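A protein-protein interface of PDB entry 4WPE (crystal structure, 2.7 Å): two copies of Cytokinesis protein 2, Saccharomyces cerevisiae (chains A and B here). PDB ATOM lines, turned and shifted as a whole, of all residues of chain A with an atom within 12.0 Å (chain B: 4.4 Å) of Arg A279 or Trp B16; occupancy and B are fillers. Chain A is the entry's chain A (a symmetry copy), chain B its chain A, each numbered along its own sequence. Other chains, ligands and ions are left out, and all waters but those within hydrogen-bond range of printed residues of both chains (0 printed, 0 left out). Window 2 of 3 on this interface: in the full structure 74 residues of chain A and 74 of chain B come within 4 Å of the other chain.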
ATOM      1  N   ILE A 268      10.630   6.996 -26.534  1.00  0.00           N
ATOM      2  CA  ILE A 268      11.935   6.516 -26.960  1.00  0.00           C
ATOM      3  C   ILE A 268      12.199   5.122 -26.395  1.00  0.00           C
ATOM      4  O   ILE A 268      12.719   4.250 -27.093  1.00  0.00           O
ATOM      5  CB  ILE A 268      13.046   7.491 -26.531  1.00  0.00           C
ATOM      6  CG1 ILE A 268      12.950   8.776 -27.354  1.00  0.00           C
ATOM      7  CG2 ILE A 268      14.419   6.863 -26.712  1.00  0.00           C
ATOM      8  CD1 ILE A 268      13.674   9.948 -26.746  1.00  0.00           C
ATOM      9  N   SER A 269      11.819   4.913 -25.137  1.00  0.00           N
ATOM     10  CA  SER A 269      11.992   3.617 -24.484  1.00  0.00           C
ATOM     11  C   SER A 269      11.244   2.502 -25.208  1.00  0.00           C
ATOM     12  O   SER A 269      11.809   1.452 -25.514  1.00  0.00           O
ATOM     13  CB  SER A 269      11.521   3.681 -23.031  1.00  0.00           C
ATOM     14  OG  SER A 269      11.046   2.414 -22.600  1.00  0.00           O
ATOM     15  N   THR A 270       9.968   2.737 -25.480  1.00  0.00           N
ATOM     16  CA  THR A 270       9.126   1.720 -26.091  1.00  0.00           C
ATOM     17  C   THR A 270       9.508   1.447 -27.544  1.00  0.00           C
ATOM     18  O   THR A 270       9.528   0.297 -27.969  1.00  0.00           O
ATOM     19  CB  THR A 270       7.640   2.113 -26.017  1.00  0.00           C
ATOM     20  OG1 THR A 270       7.475   3.457 -26.488  1.00  0.00           O
ATOM     21  CG2 THR A 270       7.144   2.024 -24.582  1.00  0.00           C
ATOM     22  N   PHE A 271       9.816   2.499 -28.298  1.00  0.00           N
ATOM     23  CA  PHE A 271      10.194   2.346 -29.702  1.00  0.00           C
ATOM     24  C   PHE A 271      11.442   1.482 -29.844  1.00  0.00           C
ATOM     25  O   PHE A 271      11.528   0.643 -30.739  1.00  0.00           O
ATOM     26  CB  PHE A 271      10.427   3.713 -30.354  1.00  0.00           C
ATOM     27  CG  PHE A 271      10.692   3.645 -31.837  1.00  0.00           C
ATOM     28  CD1 PHE A 271       9.654   3.776 -32.745  1.00  0.00           C
ATOM     29  CD2 PHE A 271      11.979   3.462 -32.320  1.00  0.00           C
ATOM     30  CE1 PHE A 271       9.893   3.716 -34.107  1.00  0.00           C
ATOM     31  CE2 PHE A 271      12.224   3.401 -33.680  1.00  0.00           C
ATOM     32  CZ  PHE A 271      11.180   3.529 -34.575  1.00  0.00           C
ATOM     33  N   SER A 272      12.407   1.694 -28.956  1.00  0.00           N
ATOM     34  CA  SER A 272      13.656   0.943 -28.989  1.00  0.00           C
ATOM     35  C   SER A 272      13.417  -0.515 -28.609  1.00  0.00           C
ATOM     36  O   SER A 272      14.123  -1.413 -29.070  1.00  0.00           O
ATOM     37  CB  SER A 272      14.685   1.576 -28.052  1.00  0.00           C
ATOM     38  OG  SER A 272      14.924   2.929 -28.403  1.00  0.00           O
ATOM     39  N   LYS A 273      12.418  -0.737 -27.763  1.00  0.00           N
ATOM     40  CA  LYS A 273      12.037  -2.082 -27.349  1.00  0.00           C
ATOM     41  C   LYS A 273      11.481  -2.874 -28.526  1.00  0.00           C
ATOM     42  O   LYS A 273      11.812  -4.044 -28.713  1.00  0.00           O
ATOM     43  CB  LYS A 273      10.997  -2.019 -26.228  1.00  0.00           C
ATOM     44  CG  LYS A 273      11.388  -2.727 -24.940  1.00  0.00           C
ATOM     45  CD  LYS A 273      10.277  -2.598 -23.902  1.00  0.00           C
ATOM     46  CE  LYS A 273      10.723  -3.091 -22.534  1.00  0.00           C
ATOM     47  NZ  LYS A 273       9.618  -3.040 -21.536  1.00  0.00           N
ATOM     48  N   GLU A 274      10.637  -2.225 -29.322  1.00  0.00           N
ATOM     49  CA  GLU A 274       9.935  -2.898 -30.411  1.00  0.00           C
ATOM     50  C   GLU A 274      10.779  -3.072 -31.669  1.00  0.00           C
ATOM     51  O   GLU A 274      10.601  -4.038 -32.409  1.00  0.00           O
ATOM     52  CB  GLU A 274       8.660  -2.132 -30.772  1.00  0.00           C
ATOM     53  CG  GLU A 274       7.840  -1.680 -29.583  1.00  0.00           C
ATOM     54  CD  GLU A 274       6.659  -0.825 -29.990  1.00  0.00           C
ATOM     55  OE1 GLU A 274       6.721  -0.197 -31.068  1.00  0.00           O
ATOM     56  OE2 GLU A 274       5.671  -0.775 -29.229  1.00  0.00           O
ATOM     57  N   ASN A 275      11.692  -2.138 -31.916  1.00  0.00           N
ATOM     58  CA  ASN A 275      12.379  -2.101 -33.202  1.00  0.00           C
ATOM     59  C   ASN A 275      13.898  -2.060 -33.114  1.00  0.00           C
ATOM     60  O   ASN A 275      14.572  -1.798 -34.111  1.00  0.00           O
ATOM     61  CB  ASN A 275      11.882  -0.901 -34.011  1.00  0.00           C
ATOM     62  CG  ASN A 275      10.377  -0.885 -34.153  1.00  0.00           C
ATOM     63  OD1 ASN A 275       9.762  -1.909 -34.452  1.00  0.00           O
ATOM     64  ND2 ASN A 275       9.772   0.279 -33.938  1.00  0.00           N
ATOM     65  N   GLY A 276      14.435  -2.326 -31.928  1.00  0.00           N
ATOM     66  CA  GLY A 276      15.874  -2.379 -31.748  1.00  0.00           C
ATOM     67  C   GLY A 276      16.483  -3.514 -32.548  1.00  0.00           C
ATOM     68  O   GLY A 276      15.917  -4.603 -32.610  1.00  0.00           O
ATOM     69  N   THR A 277      17.636  -3.265 -33.164  1.00  0.00           N
ATOM     70  CA  THR A 277      18.275  -4.272 -34.009  1.00  0.00           C
ATOM     71  C   THR A 277      19.444  -4.961 -33.318  1.00  0.00           C
ATOM     72  O   THR A 277      20.271  -5.596 -33.972  1.00  0.00           O
ATOM     73  CB  THR A 277      18.786  -3.664 -35.329  1.00  0.00           C
ATOM     74  OG1 THR A 277      19.711  -2.607 -35.046  1.00  0.00           O
ATOM     75  CG2 THR A 277      17.629  -3.116 -36.140  1.00  0.00           C
ATOM     76  N   GLY A 278      19.513  -4.835 -31.999  1.00  0.00           N
ATOM     77  CA  GLY A 278      20.578  -5.468 -31.244  1.00  0.00           C
ATOM     78  C   GLY A 278      21.513  -4.462 -30.607  1.00  0.00           C
ATOM     79  O   GLY A 278      21.714  -3.363 -31.124  1.00  0.00           O
ATOM     80  N   ARG A 279      22.091  -4.843 -29.474  1.00  0.00           N
ATOM     81  CA  ARG A 279      22.970  -3.951 -28.731  1.00  0.00           C
ATOM     82  C   ARG A 279      24.423  -4.127 -29.157  1.00  0.00           C
ATOM     83  O   ARG A 279      24.716  -4.858 -30.105  1.00  0.00           O
ATOM     84  CB  ARG A 279      22.811  -4.194 -27.230  1.00  0.00           C
ATOM     85  CG  ARG A 279      21.498  -3.666 -26.675  1.00  0.00           C
ATOM     86  CD  ARG A 279      21.285  -4.057 -25.223  1.00  0.00           C
ATOM     87  NE  ARG A 279      20.135  -4.941 -25.051  1.00  0.00           N
ATOM     88  CZ  ARG A 279      18.894  -4.511 -24.844  1.00  0.00           C
ATOM     89  NH1 ARG A 279      18.647  -3.210 -24.802  1.00  0.00           N
ATOM     90  NH2 ARG A 279      17.899  -5.377 -24.692  1.00  0.00           N
ATOM     91  N   LEU A 280      25.329  -3.452 -28.457  1.00  0.00           N
ATOM     92  CA  LEU A 280      26.749  -3.506 -28.786  1.00  0.00           C
ATOM     93  C   LEU A 280      27.559  -4.216 -27.705  1.00  0.00           C
ATOM     94  O   LEU A 280      27.391  -3.947 -26.515  1.00  0.00           O
ATOM     95  CB  LEU A 280      27.298  -2.095 -29.002  1.00  0.00           C
ATOM     96  CG  LEU A 280      28.819  -1.997 -29.141  1.00  0.00           C
ATOM     97  CD1 LEU A 280      29.280  -2.646 -30.436  1.00  0.00           C
ATOM     98  CD2 LEU A 280      29.283  -0.551 -29.061  1.00  0.00           C
ATOM     99  N   LYS A 281      28.440  -5.118 -28.126  1.00  0.00           N
ATOM    100  CA  LYS A 281      29.318  -5.821 -27.199  1.00  0.00           C
ATOM    101  C   LYS A 281      30.764  -5.785 -27.682  1.00  0.00           C
ATOM    102  O   LYS A 281      31.690  -5.663 -26.882  1.00  0.00           O
ATOM    103  CB  LYS A 281      28.861  -7.270 -27.018  1.00  0.00           C
ATOM    104  N   HIS B   7      19.513  -4.485 -21.326  1.00  0.00           N
ATOM    105  CA  HIS B   7      18.362  -3.919 -20.654  1.00  0.00           C
ATOM    106  C   HIS B   7      18.154  -2.466 -21.097  1.00  0.00           C
ATOM    107  O   HIS B   7      18.258  -2.193 -22.289  1.00  0.00           O
ATOM    108  CB  HIS B   7      18.558  -4.036 -19.159  1.00  0.00           C
ATOM    109  CG  HIS B   7      17.291  -4.220 -18.405  1.00  0.00           C
ATOM    110  ND1 HIS B   7      17.243  -4.317 -17.044  1.00  0.00           N
ATOM    111  CD2 HIS B   7      16.006  -4.391 -18.844  1.00  0.00           C
ATOM    112  CE1 HIS B   7      15.998  -4.538 -16.651  1.00  0.00           C
ATOM    113  NE2 HIS B   7      15.234  -4.571 -17.731  1.00  0.00           N
ATOM    114  N   SER B   8      17.919  -1.562 -20.139  1.00  0.00           N
ATOM    115  CA  SER B   8      17.722  -0.112 -20.361  1.00  0.00           C
ATOM    116  C   SER B   8      17.690   0.358 -21.818  1.00  0.00           C
ATOM    117  O   SER B   8      18.691   0.268 -22.524  1.00  0.00           O
ATOM    118  CB  SER B   8      18.811   0.672 -19.631  1.00  0.00           C
ATOM    119  OG  SER B   8      18.619   0.650 -18.233  1.00  0.00           O
ATOM    120  N   TYR B   9      16.553   0.898 -22.244  1.00  0.00           N
ATOM    121  CA  TYR B   9      16.262   1.059 -23.667  1.00  0.00           C
ATOM    122  C   TYR B   9      16.336   2.492 -24.209  1.00  0.00           C
ATOM    123  O   TYR B   9      15.623   3.385 -23.746  1.00  0.00           O
ATOM    124  CB  TYR B   9      14.869   0.497 -23.960  1.00  0.00           C
ATOM    125  CG  TYR B   9      14.672  -0.921 -23.472  1.00  0.00           C
ATOM    126  CD1 TYR B   9      14.853  -2.005 -24.321  1.00  0.00           C
ATOM    127  CD2 TYR B   9      14.325  -1.173 -22.152  1.00  0.00           C
ATOM    128  CE1 TYR B   9      14.681  -3.302 -23.866  1.00  0.00           C
ATOM    129  CE2 TYR B   9      14.156  -2.458 -21.687  1.00  0.00           C
ATOM    130  CZ  TYR B   9      14.332  -3.518 -22.544  1.00  0.00           C
ATOM    131  OH  TYR B   9      14.154  -4.793 -22.060  1.00  0.00           O
ATOM    132  N   GLU B  12      20.738   4.940 -28.683  1.00  0.00           N
ATOM    133  CA  GLU B  12      22.166   4.662 -28.777  1.00  0.00           C
ATOM    134  C   GLU B  12      22.505   3.296 -28.203  1.00  0.00           C
ATOM    135  O   GLU B  12      23.625   2.808 -28.349  1.00  0.00           O
ATOM    136  CB  GLU B  12      22.973   5.735 -28.052  1.00  0.00           C
ATOM    137  CG  GLU B  12      22.802   5.720 -26.547  1.00  0.00           C
ATOM    138  CD  GLU B  12      23.969   6.366 -25.832  1.00  0.00           C
ATOM    139  OE1 GLU B  12      23.758   6.931 -24.739  1.00  0.00           O
ATOM    140  OE2 GLU B  12      25.099   6.303 -26.363  1.00  0.00           O
ATOM    141  N   ALA B  13      21.530   2.684 -27.544  1.00  0.00           N
ATOM    142  CA  ALA B  13      21.758   1.417 -26.868  1.00  0.00           C
ATOM    143  C   ALA B  13      21.325   0.223 -27.714  1.00  0.00           C
ATOM    144  O   ALA B  13      21.991  -0.809 -27.722  1.00  0.00           O
ATOM    145  CB  ALA B  13      21.030   1.403 -25.530  1.00  0.00           C
ATOM    146  N   CYS B  14      20.225   0.376 -28.445  1.00  0.00           N
ATOM    147  CA  CYS B  14      19.525  -0.774 -29.005  1.00  0.00           C
ATOM    148  C   CYS B  14      19.561  -0.912 -30.526  1.00  0.00           C
ATOM    149  O   CYS B  14      18.891  -1.785 -31.079  1.00  0.00           O
ATOM    150  CB  CYS B  14      18.066  -0.737 -28.558  1.00  0.00           C
ATOM    151  SG  CYS B  14      17.860  -0.732 -26.770  1.00  0.00           S
ATOM    152  N   PHE B  15      20.333  -0.076 -31.212  1.00  0.00           N
ATOM    153  CA  PHE B  15      20.314  -0.116 -32.671  1.00  0.00           C
ATOM    154  C   PHE B  15      21.683  -0.386 -33.282  1.00  0.00           C
ATOM    155  O   PHE B  15      22.139   0.344 -34.161  1.00  0.00           O
ATOM    156  CB  PHE B  15      19.729   1.185 -33.216  1.00  0.00           C
ATOM    157  CG  PHE B  15      18.285   1.380 -32.859  1.00  0.00           C
ATOM    158  CD1 PHE B  15      17.284   0.934 -33.705  1.00  0.00           C
ATOM    159  CD2 PHE B  15      17.928   1.982 -31.665  1.00  0.00           C
ATOM    160  CE1 PHE B  15      15.956   1.099 -33.375  1.00  0.00           C
ATOM    161  CE2 PHE B  15      16.600   2.152 -31.330  1.00  0.00           C
ATOM    162  CZ  PHE B  15      15.612   1.710 -32.187  1.00  0.00           C
ATOM    163  N   TRP B  16      22.318  -1.459 -32.821  1.00  0.00           N
ATOM    164  CA  TRP B  16      23.613  -1.877 -33.342  1.00  0.00           C
ATOM    165  C   TRP B  16      23.490  -3.159 -34.169  1.00  0.00           C
ATOM    166  O   TRP B  16      23.433  -4.259 -33.618  1.00  0.00           O
ATOM    167  CB  TRP B  16      24.605  -2.092 -32.199  1.00  0.00           C
ATOM    168  CG  TRP B  16      24.916  -0.866 -31.390  1.00  0.00           C
ATOM    169  CD1 TRP B  16      24.318  -0.479 -30.224  1.00  0.00           C
ATOM    170  CD2 TRP B  16      25.915   0.118 -31.672  1.00  0.00           C
ATOM    171  NE1 TRP B  16      24.878   0.690 -29.768  1.00  0.00           N
ATOM    172  CE2 TRP B  16      25.868   1.080 -30.645  1.00  0.00           C
ATOM    173  CE3 TRP B  16      26.850   0.288 -32.701  1.00  0.00           C
ATOM    174  CZ2 TRP B  16      26.708   2.189 -30.606  1.00  0.00           C
ATOM    175  CZ3 TRP B  16      27.689   1.390 -32.667  1.00  0.00           C
ATOM    176  CH2 TRP B  16      27.612   2.326 -31.626  1.00  0.00           C
ATOM    177  N   ASP B  17      23.449  -3.010 -35.490  1.00  0.00           N
ATOM    178  CA  ASP B  17      23.372  -4.153 -36.396  1.00  0.00           C
ATOM    179  C   ASP B  17      24.596  -4.193 -37.311  1.00  0.00           C
ATOM    180  O   ASP B  17      25.104  -3.144 -37.709  1.00  0.00           O
ATOM    181  CB  ASP B  17      22.087  -4.095 -37.230  1.00  0.00           C
ATOM    182  N   ILE B 209      31.829   3.216 -35.042  1.00  0.00           N
ATOM    183  CA  ILE B 209      31.314   2.864 -33.726  1.00  0.00           C
ATOM    184  C   ILE B 209      31.403   4.064 -32.792  1.00  0.00           C
ATOM    185  O   ILE B 209      30.456   4.378 -32.071  1.00  0.00           O
ATOM    186  CB  ILE B 209      32.081   1.668 -33.132  1.00  0.00           C
ATOM    187  CG1 ILE B 209      31.700   0.386 -33.877  1.00  0.00           C
ATOM    188  CG2 ILE B 209      31.791   1.521 -31.651  1.00  0.00           C
ATOM    189  CD1 ILE B 209      32.420  -0.849 -33.391  1.00  0.00           C
ATOM    190  N   TRP B 212      28.769   6.663 -34.365  1.00  0.00           N
ATOM    191  CA  TRP B 212      27.367   6.255 -34.257  1.00  0.00           C
ATOM    192  C   TRP B 212      26.870   6.277 -32.815  1.00  0.00           C
ATOM    193  O   TRP B 212      25.678   6.447 -32.562  1.00  0.00           O
ATOM    194  CB  TRP B 212      27.154   4.861 -34.852  1.00  0.00           C
ATOM    195  CG  TRP B 212      25.736   4.395 -34.732  1.00  0.00           C
ATOM    196  CD1 TRP B 212      25.274   3.351 -33.986  1.00  0.00           C
ATOM    197  CD2 TRP B 212      24.587   4.983 -35.353  1.00  0.00           C
ATOM    198  NE1 TRP B 212      23.911   3.240 -34.118  1.00  0.00           N
ATOM    199  CE2 TRP B 212      23.465   4.232 -34.952  1.00  0.00           C
ATOM    200  CE3 TRP B 212      24.399   6.067 -36.216  1.00  0.00           C
ATOM    201  CZ2 TRP B 212      22.175   4.529 -35.384  1.00  0.00           C
ATOM    202  CZ3 TRP B 212      23.117   6.362 -36.644  1.00  0.00           C
ATOM    203  CH2 TRP B 212      22.022   5.595 -36.227  1.00  0.00           C
ATOM    204  N   ALA B 213      27.787   6.107 -31.870  1.00  0.00           N
ATOM    205  CA  ALA B 213      27.448   6.195 -30.457  1.00  0.00           C
ATOM    206  C   ALA B 213      26.991   7.608 -30.119  1.00  0.00           C
ATOM    207  O   ALA B 213      26.208   7.816 -29.192  1.00  0.00           O
ATOM    208  CB  ALA B 213      28.642   5.797 -29.596  1.00  0.00           C
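O of Ile A268 sits at hydrogen-bond distance from OG of Ser A272, 2.9 Å away.
The backbone carbonyl oxygen (O) of Phe B15 is in hydrogen-bond range of the indole nitrogen (NE1) of Trp B212 (3.4 Å).
O of Glu B12 is in hydrogen-bond range of NE1 of Trp B16 (2.8 Å).
No position is printed for both chains.
Of the 19 pairs that touch across the chains among the printed residues, none has its exchanged pair printed and touching as well.
Of the 12 printed residues of chain B, 7 touch a printed residue of chain A.
Printed residues of chain B that touch a printed residue of chain A: His B7, Tyr B9, Ala B13, Cys B14, Phe B15, Trp B16 and Asp B17.
Along chain B the printed residues that touch a printed residue of chain A span positions 7 to 17.
Hydrophobic or aromatic side chains of chain A within 4 Å of the printed part of chain B: Leu A280.
Among the printed residues, no Asp or Glu carboxylate lies within 4 Å of a Lys or Arg side-chain nitrogen of the other chain.
Arg A279 touches just these residues of chain B: His B7, Tyr B9, Ala B13, Cys B14 and Trp B16.
Of chain A, only Thr A277 (3.5 Å), Gly A278 (2.6 Å), Arg A279 (3.5 Å) and Leu A280 (3.6 Å) come within 4 Å of Trp B16.
Of chain A, only Arg A279 comes within 4 Å of Ala B13.
Phe B15 touches five residues of chain A.
No residue of chain A comes within 4 Å of Ile B209.
No residue of chain A comes within 4 Å of Trp B212.
Printed residues of chain B within 4 Å of Lys A273: Tyr B9.
Printed residues of chain A within 4 Å of His B7: Arg A279 (2.7 Å).
Of the printed residues of chain B, Ser A269 touches Tyr B9.
Of the printed residues of chain B, Asn A275 touches Phe B15 (3.3 Å).
Of the printed residues of chain B, Gly A278 touches Cys B14 (3.2 Å), Phe B15 (3.6 Å) and Trp B16 (2.6 Å).
Lys A281 touches none of the printed residues of chain B.
Glu A274 touches none of the printed residues of chain B.
The nearest residue of chain B that does not touch Arg A279 is Ser B8 (4.2 Å).
The nearest residue of chain A that does not touch Trp B16 is Gly A276 (6.2 Å).
The nearest printed residue of chain B that does not touch Gly A276 is Trp B16 (6.2 Å).
The backbone carbonyl oxygen (O) of His B7 is in hydrogen-bond range of the guanidinium group (NH1) of Arg A279, at 2.7 Å.
The backbone NH (N) of Gly A278 is in hydrogen-bond range of the backbone carbonyl oxygen (O) of Cys B14, 3.2 Å away.
O of Thr A277 sits close to O of Trp B16 (3.5 Å).
N of Trp B16 sits at hydrogen-bond distance from O of Gly A278 (2.6 Å).
The side-chain sulfur (SG) of Cys B14 is in hydrogen-bond range of the guanidinium group (NH1) of Arg A279 (3.3 Å).
The backbone carbonyl oxygen (O) of Cys B14 sits at hydrogen-bond distance from the backbone NH (N) of Thr A277 (2.8 Å).
Phe B15 touches Ser A272 (CE2 to OG, 3.5 Å).
CG of Lys A273 touches CE1 of Tyr B9, at 3.5 Å.
CA of Gly A276 touches O of Cys B14, 3.1 Å away.
CA of Gly A276 touches CE1 of Phe B15 (3.8 Å).
Phe B15 touches Thr A277 (C to OG1, 3.5 Å).
Asp B17 touches Thr A277 (CB to OG1, 3.6 Å).
O of Gly A278 touches N of Phe B15, at 3.6 Å.
Arg A279 touches Tyr B9.
O of Ala B13 touches CG of Arg A279 (3.1 Å).
O of Arg A279 touches CB of Trp B16, at 3.5 Å.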
